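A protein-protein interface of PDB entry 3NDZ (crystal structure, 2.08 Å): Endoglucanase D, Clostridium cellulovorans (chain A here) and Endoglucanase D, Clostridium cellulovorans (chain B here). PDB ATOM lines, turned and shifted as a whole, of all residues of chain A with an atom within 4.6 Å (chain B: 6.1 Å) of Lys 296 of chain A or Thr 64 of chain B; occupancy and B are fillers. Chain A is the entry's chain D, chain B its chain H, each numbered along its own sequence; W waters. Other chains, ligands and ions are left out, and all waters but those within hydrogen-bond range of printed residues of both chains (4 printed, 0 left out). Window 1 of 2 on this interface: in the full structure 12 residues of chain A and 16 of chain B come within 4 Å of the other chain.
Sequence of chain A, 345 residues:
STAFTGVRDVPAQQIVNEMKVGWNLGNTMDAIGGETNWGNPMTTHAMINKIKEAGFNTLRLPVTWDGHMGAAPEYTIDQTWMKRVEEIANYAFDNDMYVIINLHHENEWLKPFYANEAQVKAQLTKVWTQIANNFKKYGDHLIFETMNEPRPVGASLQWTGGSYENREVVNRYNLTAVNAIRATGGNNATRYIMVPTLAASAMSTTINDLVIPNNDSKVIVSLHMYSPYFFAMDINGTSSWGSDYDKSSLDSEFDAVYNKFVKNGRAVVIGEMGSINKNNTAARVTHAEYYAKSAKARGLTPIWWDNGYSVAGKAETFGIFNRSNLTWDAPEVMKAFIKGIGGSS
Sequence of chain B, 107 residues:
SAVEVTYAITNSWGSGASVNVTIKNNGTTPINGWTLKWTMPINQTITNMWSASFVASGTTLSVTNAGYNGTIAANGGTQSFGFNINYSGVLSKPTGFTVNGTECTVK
The side-chain amide nitrogen of Asn 65 of chain B is in hydrogen-bond range of the backbone carbonyl oxygen of Ala 297 of chain A (2.9 Å).
Thr 64 of chain B touches Lys 296 of chain A. Thr 35 of chain B touches Ala 297 of chain A (CG2 to CB, 3.9 Å). Thr 64 of chain B touches Ala 297 of chain A (CG2 to CA, 3.4 Å). Gly 299 of chain A touches Gly 67 of chain B.
The backbone carbonyl oxygen of Lys 20 of chain A sits at hydrogen-bond distance from the side-chain amino group of Lys 296 of chain A (2.8 Å). The side-chain amino group (NZ) of Lys 296 of chain A sits at hydrogen-bond distance from the side-chain hydroxyl (OG1) of Thr 301 of chain A, 3.1 Å away. O of Trp 34 of chain B sits at hydrogen-bond distance from ND2 of Asn 65 of chain B, at 2.9 Å. N of Thr 64 of chain B lies within hydrogen-bond range of O of Ser 53 of chain B, at 2.9 Å. The backbone NH of Gly 67 of chain B is in hydrogen-bond range of the side-chain amide oxygen of Asn 65 of chain B (2.8 Å).
Water W1 bridges the side-chain hydroxyl (OG1) of Thr 64 of chain B (2.6 Å) and the backbone carbonyl oxygen (O) of Lys 293 of chain A (2.7 Å). Water W3 lies within hydrogen-bond range of O of Lys 296 of chain A and O of Asn 65 of chain B. Water W2 bridges the backbone carbonyl oxygen (O) of Ile 341 of chain A (2.7 Å) and the side-chain hydroxyl (OG) of Ser 53 of chain B (2.8 Å). Water W4 bridges the side-chain hydroxyl (OG) of Ser 53 of chain B and the backbone carbonyl oxygen (O) of Ile 341 of chain A.
Lys 20 of chain A touches none of the printed residues of chain B. Of chain B, only Thr 64 comes within 4 Å of Lys 296 of chain A. Printed residues of chain B within 4 Å of Ala 297 of chain A: Thr 35 (3.9 Å), Thr 64 (3.4 Å) and Asn 65 (2.9 Å). Printed residues of chain B within 4 Å of Gly 299 of chain A: Gly 67 (3.97 Å). Phe 54 of chain B touches none of the printed residues of chain A. Thr 64 of chain B touches two residues of chain A. Printed residues of chain A within 4 Å of Asn 65 of chain B: Ala 297 (2.9 Å). The nearest printed residue of chain A that does not touch Thr 64 of chain B is Lys 293 of chain A (5.1 Å).
Hydrophobic or aromatic side chains of chain A that line the printed part of chain B: Ala 297. Printed residues of chain B that touch a printed residue of chain A: Thr 35, Thr 64, Asn 65 and Gly 67. Among the printed residues, no Asp or Glu carboxylate lies within 4 Å of a Lys or Arg side-chain nitrogen of the other chain.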
ATOM      1  N   LYS A  20       0.561   9.584  16.607  1.00  0.00           N
ATOM      2  CA  LYS A  20      -0.769   9.117  16.182  1.00  0.00           C
ATOM      3  C   LYS A  20      -1.557  10.079  15.297  1.00  0.00           C
ATOM      4  O   LYS A  20      -1.785   9.799  14.122  1.00  0.00           O
ATOM      5  CB  LYS A  20      -1.601   8.683  17.392  1.00  0.00           C
ATOM      6  CG  LYS A  20      -2.951   8.062  17.041  1.00  0.00           C
ATOM      7  CD  LYS A  20      -3.672   7.597  18.310  1.00  0.00           C
ATOM      8  CE  LYS A  20      -4.891   6.758  17.961  1.00  0.00           C
ATOM      9  NZ  LYS A  20      -5.631   6.313  19.170  1.00  0.00           N
ATOM     10  N   ALA A 292      -7.270  10.561   6.758  1.00  0.00           N
ATOM     11  CA  ALA A 292      -6.709   9.949   7.955  1.00  0.00           C
ATOM     12  C   ALA A 292      -6.344   8.481   7.718  1.00  0.00           C
ATOM     13  O   ALA A 292      -5.231   8.054   8.010  1.00  0.00           O
ATOM     14  CB  ALA A 292      -7.680  10.084   9.136  1.00  0.00           C
ATOM     15  N   LYS A 293      -7.271   7.704   7.174  1.00  0.00           N
ATOM     16  CA  LYS A 293      -6.988   6.290   6.973  1.00  0.00           C
ATOM     17  C   LYS A 293      -5.984   6.000   5.844  1.00  0.00           C
ATOM     18  O   LYS A 293      -5.176   5.075   5.951  1.00  0.00           O
ATOM     19  CB  LYS A 293      -8.273   5.461   6.872  1.00  0.00           C
ATOM     20  CG  LYS A 293      -9.032   5.583   5.599  1.00  0.00           C
ATOM     21  CD  LYS A 293     -10.345   4.794   5.704  1.00  0.00           C
ATOM     22  CE  LYS A 293     -10.792   4.321   4.323  1.00  0.00           C
ATOM     23  NZ  LYS A 293     -12.165   3.740   4.326  1.00  0.00           N
ATOM     24  N   SER A 294      -6.002   6.814   4.792  1.00  0.00           N
ATOM     25  CA  SER A 294      -5.042   6.670   3.696  1.00  0.00           C
ATOM     26  C   SER A 294      -3.619   7.050   4.136  1.00  0.00           C
ATOM     27  O   SER A 294      -2.648   6.356   3.808  1.00  0.00           O
ATOM     28  CB  SER A 294      -5.468   7.522   2.494  1.00  0.00           C
ATOM     29  OG  SER A 294      -4.558   7.407   1.408  1.00  0.00           O
ATOM     30  N   ALA A 295      -3.497   8.154   4.871  1.00  0.00           N
ATOM     31  CA  ALA A 295      -2.203   8.582   5.415  1.00  0.00           C
ATOM     32  C   ALA A 295      -1.635   7.543   6.381  1.00  0.00           C
ATOM     33  O   ALA A 295      -0.449   7.201   6.328  1.00  0.00           O
ATOM     34  CB  ALA A 295      -2.345   9.931   6.139  1.00  0.00           C
ATOM     35  N   LYS A 296      -2.490   7.060   7.281  1.00  0.00           N
ATOM     36  CA  LYS A 296      -2.066   6.109   8.292  1.00  0.00           C
ATOM     37  C   LYS A 296      -1.620   4.786   7.661  1.00  0.00           C
ATOM     38  O   LYS A 296      -0.714   4.121   8.171  1.00  0.00           O
ATOM     39  CB  LYS A 296      -3.194   5.882   9.305  1.00  0.00           C
ATOM     40  CG  LYS A 296      -2.781   5.096  10.543  1.00  0.00           C
ATOM     41  CD  LYS A 296      -1.574   5.727  11.267  1.00  0.00           C
ATOM     42  CE  LYS A 296      -1.845   7.146  11.757  1.00  0.00           C
ATOM     43  NZ  LYS A 296      -0.790   7.594  12.724  1.00  0.00           N
ATOM     44  N   ALA A 297      -2.264   4.408   6.560  1.00  0.00           N
ATOM     45  CA  ALA A 297      -1.878   3.208   5.804  1.00  0.00           C
ATOM     46  C   ALA A 297      -0.470   3.326   5.228  1.00  0.00           C
ATOM     47  O   ALA A 297       0.147   2.326   4.871  1.00  0.00           O
ATOM     48  CB  ALA A 297      -2.898   2.906   4.676  1.00  0.00           C
ATOM     49  N   ARG A 298       0.034   4.553   5.133  1.00  0.00           N
ATOM     50  CA  ARG A 298       1.410   4.768   4.694  1.00  0.00           C
ATOM     51  C   ARG A 298       2.337   5.192   5.832  1.00  0.00           C
ATOM     52  O   ARG A 298       3.392   5.774   5.597  1.00  0.00           O
ATOM     53  CB  ARG A 298       1.454   5.783   3.567  1.00  0.00           C
ATOM     54  CG  ARG A 298       0.976   5.207   2.248  1.00  0.00           C
ATOM     55  CD  ARG A 298      -0.416   5.666   1.938  1.00  0.00           C
ATOM     56  NE  ARG A 298      -0.881   5.109   0.680  1.00  0.00           N
ATOM     57  CZ  ARG A 298      -2.102   4.615   0.497  1.00  0.00           C
ATOM     58  NH1 ARG A 298      -2.979   4.615   1.501  1.00  0.00           N
ATOM     59  NH2 ARG A 298      -2.437   4.117  -0.683  1.00  0.00           N
ATOM     60  N   GLY A 299       1.922   4.901   7.062  1.00  0.00           N
ATOM     61  CA  GLY A 299       2.739   5.155   8.234  1.00  0.00           C
ATOM     62  C   GLY A 299       2.839   6.622   8.582  1.00  0.00           C
ATOM     63  O   GLY A 299       3.671   7.015   9.391  1.00  0.00           O
ATOM     64  N   LEU A 300       1.984   7.435   7.970  1.00  0.00           N
ATOM     65  CA  LEU A 300       2.038   8.877   8.174  1.00  0.00           C
ATOM     66  C   LEU A 300       1.119   9.328   9.315  1.00  0.00           C
ATOM     67  O   LEU A 300      -0.013   8.845   9.442  1.00  0.00           O
ATOM     68  CB  LEU A 300       1.650   9.604   6.888  1.00  0.00           C
ATOM     69  CG  LEU A 300       2.379   9.144   5.630  1.00  0.00           C
ATOM     70  CD1 LEU A 300       1.858   9.886   4.382  1.00  0.00           C
ATOM     71  CD2 LEU A 300       3.889   9.321   5.810  1.00  0.00           C
ATOM     72  N   THR A 301       1.602  10.256  10.133  1.00  0.00           N
ATOM     73  CA  THR A 301       0.776  10.873  11.169  1.00  0.00           C
ATOM     74  C   THR A 301       0.418  12.281  10.732  1.00  0.00           C
ATOM     75  O   THR A 301       1.297  13.113  10.535  1.00  0.00           O
ATOM     76  CB  THR A 301       1.498  10.904  12.520  1.00  0.00           C
ATOM     77  OG1 THR A 301       1.494   9.586  13.075  1.00  0.00           O
ATOM     78  CG2 THR A 301       0.791  11.835  13.506  1.00  0.00           C
ATOM     79  N   PRO A 302      -0.881  12.544  10.544  1.00  0.00           N
ATOM     80  CA  PRO A 302      -1.337  13.864  10.100  1.00  0.00           C
ATOM     81  C   PRO A 302      -1.726  14.774  11.267  1.00  0.00           C
ATOM     82  O   PRO A 302      -2.183  14.304  12.301  1.00  0.00           O
ATOM     83  CB  PRO A 302      -2.570  13.531   9.260  1.00  0.00           C
ATOM     84  CG  PRO A 302      -3.080  12.195   9.836  1.00  0.00           C
ATOM     85  CD  PRO A 302      -1.990  11.588  10.689  1.00  0.00           C
ATOM     86  N   ILE A 341      -8.325   7.494  11.856  1.00  0.00           N
ATOM     87  CA  ILE A 341      -6.996   7.195  12.389  1.00  0.00           C
ATOM     88  C   ILE A 341      -6.957   5.824  13.075  1.00  0.00           C
ATOM     89  O   ILE A 341      -5.948   5.128  13.046  1.00  0.00           O
ATOM     90  CB  ILE A 341      -6.551   8.269  13.405  1.00  0.00           C
ATOM     91  CG1 ILE A 341      -6.326   9.617  12.710  1.00  0.00           C
ATOM     92  CG2 ILE A 341      -5.307   7.816  14.165  1.00  0.00           C
ATOM     93  CD1 ILE A 341      -5.127   9.646  11.759  1.00  0.00           C
ATOM     94  N   TRP B  34       0.171  -2.132   3.558  1.00  0.00           N
ATOM     95  CA  TRP B  34      -0.935  -3.096   3.616  1.00  0.00           C
ATOM     96  C   TRP B  34      -2.071  -2.742   4.573  1.00  0.00           C
ATOM     97  O   TRP B  34      -1.868  -2.128   5.629  1.00  0.00           O
ATOM     98  CB  TRP B  34      -0.427  -4.504   3.934  1.00  0.00           C
ATOM     99  CG  TRP B  34       0.183  -4.684   5.317  1.00  0.00           C
ATOM    100  CD1 TRP B  34       1.516  -4.670   5.637  1.00  0.00           C
ATOM    101  CD2 TRP B  34      -0.519  -4.935   6.547  1.00  0.00           C
ATOM    102  NE1 TRP B  34       1.679  -4.890   6.982  1.00  0.00           N
ATOM    103  CE2 TRP B  34       0.448  -5.051   7.564  1.00  0.00           C
ATOM    104  CE3 TRP B  34      -1.870  -5.050   6.884  1.00  0.00           C
ATOM    105  CZ2 TRP B  34       0.110  -5.278   8.891  1.00  0.00           C
ATOM    106  CZ3 TRP B  34      -2.203  -5.286   8.188  1.00  0.00           C
ATOM    107  CH2 TRP B  34      -1.220  -5.396   9.184  1.00  0.00           C
ATOM    108  N   THR B  35      -3.274  -3.157   4.188  1.00  0.00           N
ATOM    109  CA  THR B  35      -4.445  -3.051   5.036  1.00  0.00           C
ATOM    110  C   THR B  35      -5.204  -4.364   4.922  1.00  0.00           C
ATOM    111  O   THR B  35      -5.268  -4.960   3.845  1.00  0.00           O
ATOM    112  CB  THR B  35      -5.360  -1.902   4.589  1.00  0.00           C
ATOM    113  OG1 THR B  35      -5.719  -2.102   3.215  1.00  0.00           O
ATOM    114  CG2 THR B  35      -4.646  -0.555   4.735  1.00  0.00           C
ATOM    115  N   LEU B  36      -5.755  -4.826   6.035  1.00  0.00           N
ATOM    116  CA  LEU B  36      -6.440  -6.114   6.079  1.00  0.00           C
ATOM    117  C   LEU B  36      -7.836  -5.917   6.646  1.00  0.00           C
ATOM    118  O   LEU B  36      -8.013  -5.267   7.673  1.00  0.00           O
ATOM    119  CB  LEU B  36      -5.653  -7.104   6.936  1.00  0.00           C
ATOM    120  CG  LEU B  36      -6.248  -8.498   7.138  1.00  0.00           C
ATOM    121  CD1 LEU B  36      -6.161  -9.300   5.855  1.00  0.00           C
ATOM    122  CD2 LEU B  36      -5.500  -9.205   8.244  1.00  0.00           C
ATOM    123  N   MET B  49      -4.163  -4.394  20.395  1.00  0.00           N
ATOM    124  CA  MET B  49      -3.480  -4.863  19.195  1.00  0.00           C
ATOM    125  C   MET B  49      -2.051  -4.311  19.131  1.00  0.00           C
ATOM    126  O   MET B  49      -1.811  -3.163  19.507  1.00  0.00           O
ATOM    127  CB  MET B  49      -4.264  -4.415  17.956  1.00  0.00           C
ATOM    128  CG  MET B  49      -3.674  -4.875  16.627  1.00  0.00           C
ATOM    129  SD  MET B  49      -4.671  -4.427  15.199  1.00  0.00           S
ATOM    130  CE  MET B  49      -6.092  -5.505  15.397  1.00  0.00           C
ATOM    131  N   SER B  51       1.663  -4.047  16.593  1.00  0.00           N
ATOM    132  CA  SER B  51       2.254  -4.122  15.254  1.00  0.00           C
ATOM    133  C   SER B  51       1.256  -3.751  14.170  1.00  0.00           C
ATOM    134  O   SER B  51       1.502  -3.960  12.982  1.00  0.00           O
ATOM    135  CB  SER B  51       2.822  -5.511  14.982  1.00  0.00           C
ATOM    136  OG  SER B  51       3.763  -5.858  15.973  1.00  0.00           O
ATOM    137  N   ALA B  52       0.135  -3.184  14.599  1.00  0.00           N
ATOM    138  CA  ALA B  52      -0.932  -2.764  13.708  1.00  0.00           C
ATOM    139  C   ALA B  52      -1.913  -1.957  14.543  1.00  0.00           C
ATOM    140  O   ALA B  52      -1.857  -1.989  15.774  1.00  0.00           O
ATOM    141  CB  ALA B  52      -1.621  -3.975  13.105  1.00  0.00           C
ATOM    142  N   SER B  53      -2.770  -1.197  13.877  1.00  0.00           N
ATOM    143  CA  SER B  53      -3.870  -0.510  14.539  1.00  0.00           C
ATOM    144  C   SER B  53      -5.126  -0.885  13.764  1.00  0.00           C
ATOM    145  O   SER B  53      -5.040  -1.403  12.646  1.00  0.00           O
ATOM    146  CB  SER B  53      -3.667   1.004  14.534  1.00  0.00           C
ATOM    147  OG  SER B  53      -3.783   1.531  13.217  1.00  0.00           O
ATOM    148  N   PHE B  54      -6.289  -0.640  14.352  1.00  0.00           N
ATOM    149  CA  PHE B  54      -7.528  -1.042  13.707  1.00  0.00           C
ATOM    150  C   PHE B  54      -8.667  -0.055  13.900  1.00  0.00           C
ATOM    151  O   PHE B  54      -8.672   0.746  14.839  1.00  0.00           O
ATOM    152  CB  PHE B  54      -7.966  -2.420  14.204  1.00  0.00           C
ATOM    153  CG  PHE B  54      -8.481  -2.431  15.623  1.00  0.00           C
ATOM    154  CD1 PHE B  54      -9.844  -2.417  15.883  1.00  0.00           C
ATOM    155  CD2 PHE B  54      -7.608  -2.481  16.690  1.00  0.00           C
ATOM    156  CE1 PHE B  54     -10.326  -2.458  17.190  1.00  0.00           C
ATOM    157  CE2 PHE B  54      -8.080  -2.517  18.001  1.00  0.00           C
ATOM    158  CZ  PHE B  54      -9.443  -2.499  18.247  1.00  0.00           C
ATOM    159  N   SER B  62     -11.077  -3.252  10.210  1.00  0.00           N
ATOM    160  CA  SER B  62     -10.065  -2.812   9.264  1.00  0.00           C
ATOM    161  C   SER B  62      -8.752  -2.610   9.990  1.00  0.00           C
ATOM    162  O   SER B  62      -8.656  -1.800  10.914  1.00  0.00           O
ATOM    163  CB  SER B  62     -10.498  -1.521   8.568  1.00  0.00           C
ATOM    164  OG  SER B  62     -11.761  -1.701   7.956  1.00  0.00           O
ATOM    165  N   VAL B  63      -7.747  -3.372   9.582  1.00  0.00           N
ATOM    166  CA  VAL B  63      -6.450  -3.341  10.231  1.00  0.00           C
ATOM    167  C   VAL B  63      -5.440  -2.689   9.293  1.00  0.00           C
ATOM    168  O   VAL B  63      -5.406  -2.973   8.103  1.00  0.00           O
ATOM    169  CB  VAL B  63      -5.994  -4.758  10.628  1.00  0.00           C
ATOM    170  CG1 VAL B  63      -4.605  -4.739  11.283  1.00  0.00           C
ATOM    171  CG2 VAL B  63      -7.002  -5.388  11.577  1.00  0.00           C
ATOM    172  N   THR B  64      -4.625  -1.805   9.839  1.00  0.00           N
ATOM    173  CA  THR B  64      -3.654  -1.083   9.055  1.00  0.00           C
ATOM    174  C   THR B  64      -2.273  -1.359   9.649  1.00  0.00           C
ATOM    175  O   THR B  64      -2.123  -1.487  10.867  1.00  0.00           O
ATOM    176  CB  THR B  64      -3.970   0.437   9.067  1.00  0.00           C
ATOM    177  OG1 THR B  64      -5.244   0.678   8.440  1.00  0.00           O
ATOM    178  CG2 THR B  64      -2.904   1.211   8.329  1.00  0.00           C
ATOM    179  N   ASN B  65      -1.275  -1.468   8.783  1.00  0.00           N
ATOM    180  CA  ASN B  65       0.109  -1.673   9.196  1.00  0.00           C
ATOM    181  C   ASN B  65       0.632  -0.563  10.116  1.00  0.00           C
ATOM    182  O   ASN B  65       0.028   0.507  10.225  1.00  0.00           O
ATOM    183  CB  ASN B  65       1.001  -1.777   7.955  1.00  0.00           C
ATOM    184  CG  ASN B  65       1.140  -0.448   7.225  1.00  0.00           C
ATOM    185  OD1 ASN B  65       1.961   0.397   7.598  1.00  0.00           O
ATOM    186  ND2 ASN B  65       0.350  -0.262   6.171  1.00  0.00           N
ATOM    187  N   ALA B  66       1.769  -0.818  10.752  1.00  0.00           N
ATOM    188  CA  ALA B  66       2.381   0.137  11.670  1.00  0.00           C
ATOM    189  C   ALA B  66       3.580   0.879  11.047  1.00  0.00           C
ATOM    190  O   ALA B  66       4.479   1.335  11.758  1.00  0.00           O
ATOM    191  CB  ALA B  66       2.794  -0.571  12.959  1.00  0.00           C
ATOM    192  N   GLY B  67       3.609   0.978   9.723  1.00  0.00           N
ATOM    193  CA  GLY B  67       4.636   1.772   9.061  1.00  0.00           C
ATOM    194  C   GLY B  67       5.920   1.010   8.785  1.00  0.00           C
ATOM    195  O   GLY B  67       6.258   0.780   7.622  1.00  0.00           O
ATOM    196  N   ASN B  69       6.412  -2.036   9.152  1.00  0.00           N
ATOM    197  CA  ASN B  69       6.070  -3.317   8.545  1.00  0.00           C
ATOM    198  C   ASN B  69       5.047  -3.149   7.408  1.00  0.00           C
ATOM    199  O   ASN B  69       4.238  -4.039   7.158  1.00  0.00           O
ATOM    200  CB  ASN B  69       5.526  -4.277   9.614  1.00  0.00           C
ATOM    201  CG  ASN B  69       4.237  -3.767  10.256  1.00  0.00           C
ATOM    202  OD1 ASN B  69       3.744  -2.691   9.914  1.00  0.00           O
ATOM    203  ND2 ASN B  69       3.685  -4.541  11.174  1.00  0.00           N
HETATM  204  O   HOH W   1      -5.907   2.984   7.468  1.00  0.00           O
HETATM  205  O   HOH W   2      -3.628   4.193  14.098  1.00  0.00           O
HETATM  206  O   HOH W   3       0.785   3.207  10.119  1.00  0.00           O
HETATM  207  O   HOH W   4      -6.299   2.141  12.153  1.00  0.00           O
